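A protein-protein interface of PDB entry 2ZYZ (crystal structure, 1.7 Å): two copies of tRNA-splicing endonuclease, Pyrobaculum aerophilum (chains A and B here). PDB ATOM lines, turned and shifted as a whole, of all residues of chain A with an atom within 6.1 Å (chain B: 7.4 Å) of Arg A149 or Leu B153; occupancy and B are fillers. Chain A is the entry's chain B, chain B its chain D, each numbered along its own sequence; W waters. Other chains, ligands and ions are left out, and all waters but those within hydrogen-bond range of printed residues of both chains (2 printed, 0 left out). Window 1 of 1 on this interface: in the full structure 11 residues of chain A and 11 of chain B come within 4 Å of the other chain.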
ATOM      1  N   VAL A 134      -2.465  18.990   9.782  1.00  0.00           N
ATOM      2  CA  VAL A 134      -1.632  19.304  10.911  1.00  0.00           C
ATOM      3  C   VAL A 134      -2.265  18.631  12.111  1.00  0.00           C
ATOM      4  O   VAL A 134      -3.425  18.655  12.195  1.00  0.00           O
ATOM      5  CB  VAL A 134      -1.610  20.812  11.157  1.00  0.00           C
ATOM      6  CG1 VAL A 134      -1.084  21.138  12.459  1.00  0.00           C
ATOM      7  CG2 VAL A 134      -0.848  21.477  10.111  1.00  0.00           C
ATOM      8  N   ALA A 144      -2.832  31.998  18.018  1.00  0.00           N
ATOM      9  CA  ALA A 144      -2.742  32.615  16.726  1.00  0.00           C
ATOM     10  C   ALA A 144      -1.584  32.098  15.888  1.00  0.00           C
ATOM     11  O   ALA A 144      -1.712  31.965  14.721  1.00  0.00           O
ATOM     12  CB  ALA A 144      -2.650  34.121  16.860  1.00  0.00           C
ATOM     13  N   THR A 145      -0.469  31.850  16.513  1.00  0.00           N
ATOM     14  CA  THR A 145       0.708  31.486  15.773  1.00  0.00           C
ATOM     15  C   THR A 145       0.556  30.121  15.112  1.00  0.00           C
ATOM     16  O   THR A 145       1.093  29.881  14.119  1.00  0.00           O
ATOM     17  CB  THR A 145       1.922  31.508  16.688  1.00  0.00           C
ATOM     18  OG1 THR A 145       2.089  32.820  17.202  1.00  0.00           O
ATOM     19  CG2 THR A 145       3.154  31.084  16.005  1.00  0.00           C
ATOM     20  N   ASP A 146      -0.206  29.230  15.710  1.00  0.00           N
ATOM     21  CA  ASP A 146      -0.514  27.967  15.072  1.00  0.00           C
ATOM     22  C   ASP A 146      -1.245  28.147  13.748  1.00  0.00           C
ATOM     23  O   ASP A 146      -1.072  27.392  12.870  1.00  0.00           O
ATOM     24  CB  ASP A 146      -1.348  27.069  15.987  1.00  0.00           C
ATOM     25  CG  ASP A 146      -0.622  26.721  17.274  1.00  0.00           C
ATOM     26  OD1 ASP A 146       0.567  26.536  17.220  1.00  0.00           O
ATOM     27  OD2 ASP A 146      -1.197  26.675  18.339  1.00  0.00           O
ATOM     28  N   ILE A 147      -2.077  29.146  13.709  1.00  0.00           N
ATOM     29  CA  ILE A 147      -2.892  29.386  12.566  1.00  0.00           C
ATOM     30  C   ILE A 147      -2.140  29.955  11.371  1.00  0.00           C
ATOM     31  O   ILE A 147      -2.252  29.477  10.287  1.00  0.00           O
ATOM     32  CB  ILE A 147      -4.168  30.120  12.949  1.00  0.00           C
ATOM     33  CG1 ILE A 147      -4.940  29.250  13.952  1.00  0.00           C
ATOM     34  CG2 ILE A 147      -4.986  30.434  11.795  1.00  0.00           C
ATOM     35  CD1 ILE A 147      -5.680  29.961  14.759  1.00  0.00           C
ATOM     36  N   THR A 148      -1.325  30.948  11.617  1.00  0.00           N
ATOM     37  CA  THR A 148      -0.450  31.425  10.562  1.00  0.00           C
ATOM     38  C   THR A 148       0.596  30.393  10.119  1.00  0.00           C
ATOM     39  O   THR A 148       1.007  30.377   8.994  1.00  0.00           O
ATOM     40  CB  THR A 148       0.258  32.728  10.930  1.00  0.00           C
ATOM     41  OG1 THR A 148       0.905  32.537  12.141  1.00  0.00           O
ATOM     42  CG2 THR A 148      -0.694  33.798  11.057  1.00  0.00           C
ATOM     43  N   ARG A 149       1.033  29.561  11.031  1.00  0.00           N
ATOM     44  CA  ARG A 149       1.974  28.534  10.696  1.00  0.00           C
ATOM     45  C   ARG A 149       1.306  27.572   9.719  1.00  0.00           C
ATOM     46  O   ARG A 149       1.854  27.257   8.738  1.00  0.00           O
ATOM     47  CB  ARG A 149       2.450  27.781  11.942  1.00  0.00           C
ATOM     48  CG  ARG A 149       3.512  26.770  11.652  1.00  0.00           C
ATOM     49  CD  ARG A 149       4.203  26.315  12.873  1.00  0.00           C
ATOM     50  NE  ARG A 149       3.309  25.574  13.682  1.00  0.00           N
ATOM     51  CZ  ARG A 149       3.077  25.796  14.956  1.00  0.00           C
ATOM     52  NH1 ARG A 149       3.750  26.708  15.617  1.00  0.00           N
ATOM     53  NH2 ARG A 149       2.208  25.069  15.596  1.00  0.00           N
ATOM     54  N   GLY A 150       0.086  27.141  10.012  1.00  0.00           N
ATOM     55  CA  GLY A 150      -0.585  26.312   9.048  1.00  0.00           C
ATOM     56  C   GLY A 150      -0.749  26.971   7.680  1.00  0.00           C
ATOM     57  O   GLY A 150      -0.612  26.354   6.707  1.00  0.00           O
ATOM     58  N   GLY A 151      -1.047  28.230   7.689  1.00  0.00           N
ATOM     59  CA  GLY A 151      -1.157  28.953   6.454  1.00  0.00           C
ATOM     60  C   GLY A 151       0.110  28.946   5.636  1.00  0.00           C
ATOM     61  O   GLY A 151       0.073  28.891   4.447  1.00  0.00           O
ATOM     62  N   ARG A 152       1.222  28.965   6.323  1.00  0.00           N
ATOM     63  CA  ARG A 152       2.523  28.863   5.685  1.00  0.00           C
ATOM     64  C   ARG A 152       2.858  27.499   5.121  1.00  0.00           C
ATOM     65  O   ARG A 152       3.486  27.391   4.125  1.00  0.00           O
ATOM     66  CB  ARG A 152       3.661  29.373   6.573  1.00  0.00           C
ATOM     67  CG  ARG A 152       5.036  29.181   6.041  1.00  0.00           C
ATOM     68  CD  ARG A 152       5.392  30.130   4.867  1.00  0.00           C
ATOM     69  NE  ARG A 152       6.798  30.061   4.560  1.00  0.00           N
ATOM     70  CZ  ARG A 152       7.384  30.697   3.571  1.00  0.00           C
ATOM     71  NH1 ARG A 152       6.693  31.493   2.809  1.00  0.00           N
ATOM     72  NH2 ARG A 152       8.658  30.560   3.393  1.00  0.00           N
ATOM     73  N   LEU A 153       2.430  26.464   5.814  1.00  0.00           N
ATOM     74  CA  LEU A 153       2.587  25.135   5.330  1.00  0.00           C
ATOM     75  C   LEU A 153       1.770  24.849   4.078  1.00  0.00           C
ATOM     76  O   LEU A 153       2.120  24.021   3.336  1.00  0.00           O
ATOM     77  CB  LEU A 153       2.263  24.135   6.416  1.00  0.00           C
ATOM     78  CG  LEU A 153       3.005  24.267   7.726  1.00  0.00           C
ATOM     79  CD1 LEU A 153       2.552  23.103   8.570  1.00  0.00           C
ATOM     80  CD2 LEU A 153       4.477  24.267   7.584  1.00  0.00           C
ATOM     81  N   SER A 154       0.669  25.560   3.930  1.00  0.00           N
ATOM     82  CA  SER A 154      -0.224  25.405   2.792  1.00  0.00           C
ATOM     83  C   SER A 154       0.507  25.636   1.472  1.00  0.00           C
ATOM     84  O   SER A 154       1.325  26.484   1.387  1.00  0.00           O
ATOM     85  CB  SER A 154      -1.370  26.408   2.828  1.00  0.00           C
ATOM     86  OG  SER A 154      -2.321  26.144   1.838  1.00  0.00           O
ATOM     87  N   TRP A 161      -5.604  24.887   5.145  1.00  0.00           N
ATOM     88  CA  TRP A 161      -4.957  23.798   5.839  1.00  0.00           C
ATOM     89  C   TRP A 161      -5.981  23.188   6.781  1.00  0.00           C
ATOM     90  O   TRP A 161      -6.943  23.783   7.055  1.00  0.00           O
ATOM     91  CB  TRP A 161      -3.692  24.234   6.627  1.00  0.00           C
ATOM     92  CG  TRP A 161      -3.911  25.186   7.745  1.00  0.00           C
ATOM     93  CD1 TRP A 161      -4.084  26.500   7.650  1.00  0.00           C
ATOM     94  CD2 TRP A 161      -3.958  24.892   9.139  1.00  0.00           C
ATOM     95  NE1 TRP A 161      -4.275  27.062   8.862  1.00  0.00           N
ATOM     96  CE2 TRP A 161      -4.167  26.086   9.806  1.00  0.00           C
ATOM     97  CE3 TRP A 161      -3.814  23.739   9.887  1.00  0.00           C
ATOM     98  CZ2 TRP A 161      -4.270  26.142  11.183  1.00  0.00           C
ATOM     99  CZ3 TRP A 161      -3.908  23.817  11.223  1.00  0.00           C
ATOM    100  CH2 TRP A 161      -4.139  24.986  11.860  1.00  0.00           C
ATOM    101  N   GLY B 110       6.830  37.080  15.862  1.00  0.00           N
ATOM    102  CA  GLY B 110       6.947  35.999  14.925  1.00  0.00           C
ATOM    103  C   GLY B 110       5.666  35.555  14.248  1.00  0.00           C
ATOM    104  O   GLY B 110       5.698  34.725  13.414  1.00  0.00           O
ATOM    105  N   LEU B 111       4.555  36.122  14.627  1.00  0.00           N
ATOM    106  CA  LEU B 111       3.256  35.677  14.143  1.00  0.00           C
ATOM    107  C   LEU B 111       3.176  35.566  12.631  1.00  0.00           C
ATOM    108  O   LEU B 111       2.753  34.590  12.141  1.00  0.00           O
ATOM    109  CB  LEU B 111       2.136  36.551  14.679  1.00  0.00           C
ATOM    110  CG  LEU B 111       0.707  36.238  14.280  1.00  0.00           C
ATOM    111  CD1 LEU B 111       0.345  34.920  14.828  1.00  0.00           C
ATOM    112  CD2 LEU B 111      -0.251  37.250  14.694  1.00  0.00           C
ATOM    113  N   LYS B 112       3.608  36.572  11.913  1.00  0.00           N
ATOM    114  CA  LYS B 112       3.511  36.474  10.474  1.00  0.00           C
ATOM    115  C   LYS B 112       4.278  35.306   9.871  1.00  0.00           C
ATOM    116  O   LYS B 112       3.957  34.861   8.844  1.00  0.00           O
ATOM    117  CB  LYS B 112       3.878  37.773   9.778  1.00  0.00           C
ATOM    118  CG  LYS B 112       5.259  38.104   9.877  1.00  0.00           C
ATOM    119  CD  LYS B 112       5.582  39.535   9.439  1.00  0.00           C
ATOM    120  CE  LYS B 112       5.374  39.762   7.962  1.00  0.00           C
ATOM    121  NZ  LYS B 112       5.923  41.090   7.505  1.00  0.00           N
ATOM    122  N   PHE B 113       5.265  34.818  10.597  1.00  0.00           N
ATOM    123  CA  PHE B 113       6.096  33.740  10.163  1.00  0.00           C
ATOM    124  C   PHE B 113       5.646  32.376  10.662  1.00  0.00           C
ATOM    125  O   PHE B 113       6.204  31.396  10.296  1.00  0.00           O
ATOM    126  CB  PHE B 113       7.552  33.967  10.562  1.00  0.00           C
ATOM    127  CG  PHE B 113       8.140  35.232   9.986  1.00  0.00           C
ATOM    128  CD1 PHE B 113       8.133  36.378  10.695  1.00  0.00           C
ATOM    129  CD2 PHE B 113       8.652  35.253   8.727  1.00  0.00           C
ATOM    130  CE1 PHE B 113       8.612  37.492  10.163  1.00  0.00           C
ATOM    131  CE2 PHE B 113       9.155  36.405   8.212  1.00  0.00           C
ATOM    132  CZ  PHE B 113       9.130  37.491   8.928  1.00  0.00           C
ATOM    133  N   GLY B 114       4.683  32.346  11.551  1.00  0.00           N
ATOM    134  CA  GLY B 114       4.322  31.111  12.214  1.00  0.00           C
ATOM    135  C   GLY B 114       5.296  30.642  13.275  1.00  0.00           C
ATOM    136  O   GLY B 114       5.380  29.487  13.592  1.00  0.00           O
ATOM    137  N   ALA B 115       5.996  31.607  13.836  1.00  0.00           N
ATOM    138  CA  ALA B 115       7.088  31.321  14.763  1.00  0.00           C
ATOM    139  C   ALA B 115       7.027  32.204  16.007  1.00  0.00           C
ATOM    140  O   ALA B 115       6.204  33.017  16.099  1.00  0.00           O
ATOM    141  CB  ALA B 115       8.403  31.462  14.097  1.00  0.00           C
ATOM    142  N   LEU B 116       7.937  32.011  16.933  1.00  0.00           N
ATOM    143  CA  LEU B 116       7.974  32.789  18.143  1.00  0.00           C
ATOM    144  C   LEU B 116       8.407  34.210  17.867  1.00  0.00           C
ATOM    145  O   LEU B 116       7.707  35.118  18.129  1.00  0.00           O
ATOM    146  CB  LEU B 116       8.898  32.189  19.193  1.00  0.00           C
ATOM    147  CG  LEU B 116       8.911  32.844  20.552  1.00  0.00           C
ATOM    148  CD1 LEU B 116       7.629  32.781  21.244  1.00  0.00           C
ATOM    149  CD2 LEU B 116       9.991  32.284  21.354  1.00  0.00           C
ATOM    150  N   VAL B 132      14.205  33.402  11.637  1.00  0.00           N
ATOM    151  CA  VAL B 132      13.045  32.826  12.211  1.00  0.00           C
ATOM    152  C   VAL B 132      13.379  31.987  13.434  1.00  0.00           C
ATOM    153  O   VAL B 132      14.103  31.091  13.334  1.00  0.00           O
ATOM    154  CB  VAL B 132      12.263  31.992  11.180  1.00  0.00           C
ATOM    155  CG1 VAL B 132      11.033  31.399  11.807  1.00  0.00           C
ATOM    156  CG2 VAL B 132      11.908  32.839  10.008  1.00  0.00           C
ATOM    157  N   VAL B 133      12.780  32.317  14.553  1.00  0.00           N
ATOM    158  CA  VAL B 133      13.078  31.668  15.778  1.00  0.00           C
ATOM    159  C   VAL B 133      11.843  30.899  16.273  1.00  0.00           C
ATOM    160  O   VAL B 133      10.869  31.475  16.514  1.00  0.00           O
ATOM    161  CB  VAL B 133      13.512  32.677  16.843  1.00  0.00           C
ATOM    162  CG1 VAL B 133      13.702  32.042  18.164  1.00  0.00           C
ATOM    163  CG2 VAL B 133      14.738  33.409  16.402  1.00  0.00           C
ATOM    164  N   VAL B 134      11.998  29.588  16.403  1.00  0.00           N
ATOM    165  CA  VAL B 134      10.953  28.699  16.821  1.00  0.00           C
ATOM    166  C   VAL B 134      11.189  28.283  18.268  1.00  0.00           C
ATOM    167  O   VAL B 134      12.276  28.069  18.582  1.00  0.00           O
ATOM    168  CB  VAL B 134      10.967  27.446  15.968  1.00  0.00           C
ATOM    169  CG1 VAL B 134      10.105  26.387  16.518  1.00  0.00           C
ATOM    170  CG2 VAL B 134      10.652  27.757  14.534  1.00  0.00           C
ATOM    171  N   PHE B 135      10.135  28.190  19.070  1.00  0.00           N
ATOM    172  CA  PHE B 135      10.214  27.885  20.509  1.00  0.00           C
ATOM    173  C   PHE B 135      10.050  26.380  20.796  1.00  0.00           C
ATOM    174  O   PHE B 135       9.189  25.763  20.292  1.00  0.00           O
ATOM    175  CB  PHE B 135       9.102  28.609  21.261  1.00  0.00           C
ATOM    176  CG  PHE B 135       9.111  28.443  22.789  1.00  0.00           C
ATOM    177  CD1 PHE B 135      10.227  28.642  23.515  1.00  0.00           C
ATOM    178  CD2 PHE B 135       7.954  28.176  23.473  1.00  0.00           C
ATOM    179  CE1 PHE B 135      10.199  28.523  24.857  1.00  0.00           C
ATOM    180  CE2 PHE B 135       7.951  28.046  24.827  1.00  0.00           C
ATOM    181  CZ  PHE B 135       9.052  28.223  25.492  1.00  0.00           C
ATOM    182  N   ASP B 146       9.303  18.439  12.907  1.00  0.00           N
ATOM    183  CA  ASP B 146       9.535  19.763  13.453  1.00  0.00           C
ATOM    184  C   ASP B 146      10.614  20.462  12.616  1.00  0.00           C
ATOM    185  O   ASP B 146      10.580  21.625  12.409  1.00  0.00           O
ATOM    186  CB  ASP B 146      10.001  19.684  14.881  1.00  0.00           C
ATOM    187  CG  ASP B 146       8.942  19.127  15.807  1.00  0.00           C
ATOM    188  OD1 ASP B 146       7.772  19.278  15.557  1.00  0.00           O
ATOM    189  OD2 ASP B 146       9.304  18.567  16.807  1.00  0.00           O
ATOM    190  N   ILE B 147      11.547  19.681  12.147  1.00  0.00           N
ATOM    191  CA  ILE B 147      12.694  20.235  11.479  1.00  0.00           C
ATOM    192  C   ILE B 147      12.375  20.663  10.059  1.00  0.00           C
ATOM    193  O   ILE B 147      12.675  21.733   9.676  1.00  0.00           O
ATOM    194  CB  ILE B 147      13.887  19.325  11.576  1.00  0.00           C
ATOM    195  CG1 ILE B 147      14.252  19.135  13.032  1.00  0.00           C
ATOM    196  CG2 ILE B 147      15.000  19.781  10.701  1.00  0.00           C
ATOM    197  CD1 ILE B 147      15.048  17.975  13.287  1.00  0.00           C
ATOM    198  N   THR B 148      11.718  19.810   9.316  1.00  0.00           N
ATOM    199  CA  THR B 148      11.186  20.238   8.057  1.00  0.00           C
ATOM    200  C   THR B 148      10.190  21.392   8.131  1.00  0.00           C
ATOM    201  O   THR B 148      10.163  22.196   7.244  1.00  0.00           O
ATOM    202  CB  THR B 148      10.579  19.098   7.267  1.00  0.00           C
ATOM    203  OG1 THR B 148       9.522  18.558   8.001  1.00  0.00           O
ATOM    204  CG2 THR B 148      11.600  18.081   6.979  1.00  0.00           C
ATOM    205  N   ARG B 149       9.370  21.406   9.157  1.00  0.00           N
ATOM    206  CA  ARG B 149       8.508  22.546   9.375  1.00  0.00           C
ATOM    207  C   ARG B 149       9.300  23.839   9.499  1.00  0.00           C
ATOM    208  O   ARG B 149       8.985  24.796   8.888  1.00  0.00           O
ATOM    209  CB  ARG B 149       7.648  22.409  10.605  1.00  0.00           C
ATOM    210  CG  ARG B 149       6.606  23.441  10.693  1.00  0.00           C
ATOM    211  CD  ARG B 149       5.507  23.009  11.591  1.00  0.00           C
ATOM    212  NE  ARG B 149       6.001  22.985  12.942  1.00  0.00           N
ATOM    213  CZ  ARG B 149       6.112  21.875  13.632  1.00  0.00           C
ATOM    214  NH1 ARG B 149       5.752  20.735  13.083  1.00  0.00           N
ATOM    215  NH2 ARG B 149       6.581  21.888  14.848  1.00  0.00           N
ATOM    216  N   GLY B 150      10.318  23.824  10.330  1.00  0.00           N
ATOM    217  CA  GLY B 150      11.083  25.039  10.482  1.00  0.00           C
ATOM    218  C   GLY B 150      11.678  25.457   9.143  1.00  0.00           C
ATOM    219  O   GLY B 150      11.721  26.593   8.844  1.00  0.00           O
ATOM    220  N   GLY B 151      12.138  24.496   8.392  1.00  0.00           N
ATOM    221  CA  GLY B 151      12.659  24.775   7.074  1.00  0.00           C
ATOM    222  C   GLY B 151      11.668  25.444   6.170  1.00  0.00           C
ATOM    223  O   GLY B 151      12.025  26.288   5.434  1.00  0.00           O
ATOM    224  N   ARG B 152      10.402  25.078   6.291  1.00  0.00           N
ATOM    225  CA  ARG B 152       9.333  25.707   5.527  1.00  0.00           C
ATOM    226  C   ARG B 152       9.013  27.117   6.021  1.00  0.00           C
ATOM    227  O   ARG B 152       8.584  27.941   5.291  1.00  0.00           O
ATOM    228  CB  ARG B 152       8.084  24.823   5.522  1.00  0.00           C
ATOM    229  CG  ARG B 152       6.882  25.436   4.925  1.00  0.00           C
ATOM    230  CD  ARG B 152       7.034  25.720   3.452  1.00  0.00           C
ATOM    231  NE  ARG B 152       5.787  26.147   2.863  1.00  0.00           N
ATOM    232  CZ  ARG B 152       5.613  26.503   1.613  1.00  0.00           C
ATOM    233  NH1 ARG B 152       6.628  26.505   0.786  1.00  0.00           N
ATOM    234  NH2 ARG B 152       4.431  26.857   1.181  1.00  0.00           N
ATOM    235  N   LEU B 153       9.198  27.359   7.297  1.00  0.00           N
ATOM    236  CA  LEU B 153       8.929  28.678   7.812  1.00  0.00           C
ATOM    237  C   LEU B 153       9.998  29.680   7.393  1.00  0.00           C
ATOM    238  O   LEU B 153       9.746  30.835   7.366  1.00  0.00           O
ATOM    239  CB  LEU B 153       8.832  28.657   9.328  1.00  0.00           C
ATOM    240  CG  LEU B 153       7.809  27.701   9.936  1.00  0.00           C
ATOM    241  CD1 LEU B 153       7.824  27.919  11.398  1.00  0.00           C
ATOM    242  CD2 LEU B 153       6.442  27.935   9.347  1.00  0.00           C
ATOM    243  N   SER B 154      11.177  29.181   7.108  1.00  0.00           N
ATOM    244  CA  SER B 154      12.282  30.022   6.739  1.00  0.00           C
ATOM    245  C   SER B 154      11.981  30.766   5.432  1.00  0.00           C
ATOM    246  O   SER B 154      11.389  30.244   4.572  1.00  0.00           O
ATOM    247  CB  SER B 154      13.503  29.170   6.472  1.00  0.00           C
ATOM    248  OG  SER B 154      14.587  29.937   6.130  1.00  0.00           O
ATOM    249  N   HIS B 155      12.480  31.973   5.349  1.00  0.00           N
ATOM    250  CA  HIS B 155      12.514  32.719   4.110  1.00  0.00           C
ATOM    251  C   HIS B 155      13.847  32.674   3.377  1.00  0.00           C
ATOM    252  O   HIS B 155      14.030  33.327   2.391  1.00  0.00           O
ATOM    253  CB  HIS B 155      12.108  34.173   4.363  1.00  0.00           C
ATOM    254  CG  HIS B 155      10.648  34.363   4.581  1.00  0.00           C
ATOM    255  ND1 HIS B 155       9.996  35.512   4.224  1.00  0.00           N
ATOM    256  CD2 HIS B 155       9.714  33.558   5.122  1.00  0.00           C
ATOM    257  CE1 HIS B 155       8.729  35.414   4.548  1.00  0.00           C
ATOM    258  NE2 HIS B 155       8.524  34.224   5.053  1.00  0.00           N
ATOM    259  N   SER B 156      14.735  31.818   3.840  1.00  0.00           N
ATOM    260  CA  SER B 156      15.965  31.572   3.143  1.00  0.00           C
ATOM    261  C   SER B 156      15.917  30.447   2.162  1.00  0.00           C
ATOM    262  O   SER B 156      15.346  29.465   2.433  1.00  0.00           O
ATOM    263  CB  SER B 156      17.072  31.300   4.126  1.00  0.00           C
ATOM    264  OG  SER B 156      18.245  30.919   3.487  1.00  0.00           O
ATOM    265  N   LYS B 159      16.830  27.395   3.833  1.00  0.00           N
ATOM    266  CA  LYS B 159      15.880  26.846   4.758  1.00  0.00           C
ATOM    267  C   LYS B 159      16.386  26.898   6.175  1.00  0.00           C
ATOM    268  O   LYS B 159      16.123  26.022   6.941  1.00  0.00           O
ATOM    269  CB  LYS B 159      15.408  25.456   4.360  1.00  0.00           C
ATOM    270  CG  LYS B 159      14.656  25.402   3.070  1.00  0.00           C
ATOM    271  CD  LYS B 159      14.004  24.119   2.784  1.00  0.00           C
ATOM    272  CE  LYS B 159      13.566  24.037   1.343  1.00  0.00           C
ATOM    273  NZ  LYS B 159      13.010  22.763   1.011  1.00  0.00           N
ATOM    274  N   THR B 160      17.126  27.944   6.460  1.00  0.00           N
ATOM    275  CA  THR B 160      17.700  28.144   7.767  1.00  0.00           C
ATOM    276  C   THR B 160      16.720  28.635   8.834  1.00  0.00           C
ATOM    277  O   THR B 160      15.915  29.463   8.587  1.00  0.00           O
ATOM    278  CB  THR B 160      18.896  29.065   7.700  1.00  0.00           C
ATOM    279  OG1 THR B 160      18.521  30.248   7.065  1.00  0.00           O
ATOM    280  CG2 THR B 160      19.978  28.444   6.927  1.00  0.00           C
ATOM    281  N   TRP B 161      16.806  28.081  10.020  1.00  0.00           N
ATOM    282  CA  TRP B 161      15.959  28.506  11.101  1.00  0.00           C
ATOM    283  C   TRP B 161      16.629  28.229  12.448  1.00  0.00           C
ATOM    284  O   TRP B 161      17.532  27.491  12.489  1.00  0.00           O
ATOM    285  CB  TRP B 161      14.565  27.888  11.017  1.00  0.00           C
ATOM    286  CG  TRP B 161      14.543  26.405  11.204  1.00  0.00           C
ATOM    287  CD1 TRP B 161      14.818  25.477  10.269  1.00  0.00           C
ATOM    288  CD2 TRP B 161      14.216  25.687  12.392  1.00  0.00           C
ATOM    289  NE1 TRP B 161      14.730  24.230  10.793  1.00  0.00           N
ATOM    290  CE2 TRP B 161      14.343  24.334  12.099  1.00  0.00           C
ATOM    291  CE3 TRP B 161      13.824  26.055  13.664  1.00  0.00           C
ATOM    292  CZ2 TRP B 161      14.108  23.362  13.051  1.00  0.00           C
ATOM    293  CZ3 TRP B 161      13.582  25.089  14.585  1.00  0.00           C
ATOM    294  CH2 TRP B 161      13.736  23.772  14.289  1.00  0.00           C
HETATM  295  O   HOH W   1       4.351  34.038  17.773  1.00  0.00           O
HETATM  296  O   HOH W   2       6.676  27.531  14.963  1.00  0.00           O
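The backbone carbonyl oxygen (O) of Thr A145 is in hydrogen-bond range of the side-chain hydroxyl (OG1) of Thr A148. OD1 of Asp A146 is in salt-bridge range of NH2 of Arg A149 (2.7 Å). The backbone carbonyl oxygen of Gly B110 is in hydrogen-bond range of the backbone NH of Ala B115 (3.2 Å). The side-chain carboxylate of Asp B146 lies within salt-bridge range of the guanidinium group of Arg B149, 3.0 Å away. OG of Ser B154 sits at hydrogen-bond distance from N of Ser B156 (3.0 Å). OG of Ser B154 is in hydrogen-bond range of O of Thr B160, at 2.8 Å.
Thr A145 touches Leu B111 (CA to CD1, 3.6 Å). Thr A145 touches Gly B114 (CG2 to C, 3.5 Å). Thr A145 touches Ala B115 (CG2 to O, 3.6 Å). Thr A148 touches Gly B114 (OG1 to CA, 3.7 Å). Arg A149 touches Arg B149 (CD to CD, 3.8 Å). Arg A149 touches Leu B153. Arg A152 touches Leu B153 (CG to CD2, 3.8 Å). NH2 of Arg A152 touches CD2 of His B155 (3.6 Å). CD2 of Leu A153 touches CG of Arg B149, 3.9 Å away. CG of Arg B152 touches CD2 of Leu A153, at 3.8 Å.
Water W1 lies within hydrogen-bond range of the side-chain hydroxyl of Thr A145 (2.6 Å) and the backbone carbonyl oxygen of Ala B115 (2.7 Å). Water W2 lies within hydrogen-bond range of O of Gly B114 (2.7 Å) and NH1 of Arg A149 (3.1 Å).
Arg A149 touches its own counterpart, Arg B149. Arg A149 touches Leu B153, and with the chains exchanged Leu A153 touches Arg B149. Arg B152 touches its own counterpart, Arg A152. Arg A152 touches Ser B154, and with the chains exchanged Ser A154 touches Arg B152. Of the 16 pairs that touch across the chains among the printed residues, 8 have their exchanged pair printed and touching as well.
The backbone carbonyl oxygen of Leu B111 sits at hydrogen-bond distance from the side-chain hydroxyl of Thr A148 (2.8 Å). O of Arg B152 lies within hydrogen-bond range of NE of Arg A152. The backbone carbonyl oxygen (O) of Ser B154 lies within hydrogen-bond range of the guanidinium group (NH2) of Arg A152, at 3.0 Å. O of Ser A154 lies within hydrogen-bond range of NH2 of Arg B152 (3.1 Å).
Of the 13 printed residues of chain A, 7 touch a printed residue of chain B. Printed residues of chain A that touch a printed residue of chain B: Ala A144, Thr A145, Thr A148, Arg A149, Arg A152, Leu A153 and Ser A154. Of the 25 printed residues of chain B, 8 touch a printed residue of chain A. Among the printed residues, 16 pairs touch across the chains. Among the printed residues, no Asp or Glu carboxylate lies within 4 Å of a Lys or Arg side-chain nitrogen of the other chain.
Of the printed residues of chain B, Ala A144 touches Leu B111. Printed residues of chain A within 4 Å of Leu B111: Ala A144, Thr A145 and Thr A148. Of the printed residues of chain A, Gly B114 touches Thr A145 (3.5 Å), Thr A148 (3.7 Å) and Arg A149 (3.5 Å). Printed residues of chain A within 4 Å of Arg B149: Arg A149 (3.8 Å) and Leu A153 (3.9 Å). Gly B151 touches none of the printed residues of chain A. Of the printed residues of chain A, Ser B154 touches Arg A152. The nearest residue of chain A that does not touch Leu B153 is Leu A153 (4.5 Å). The nearest printed residue of chain A that does not touch Gly B114 is Arg A152 (5.9 Å).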
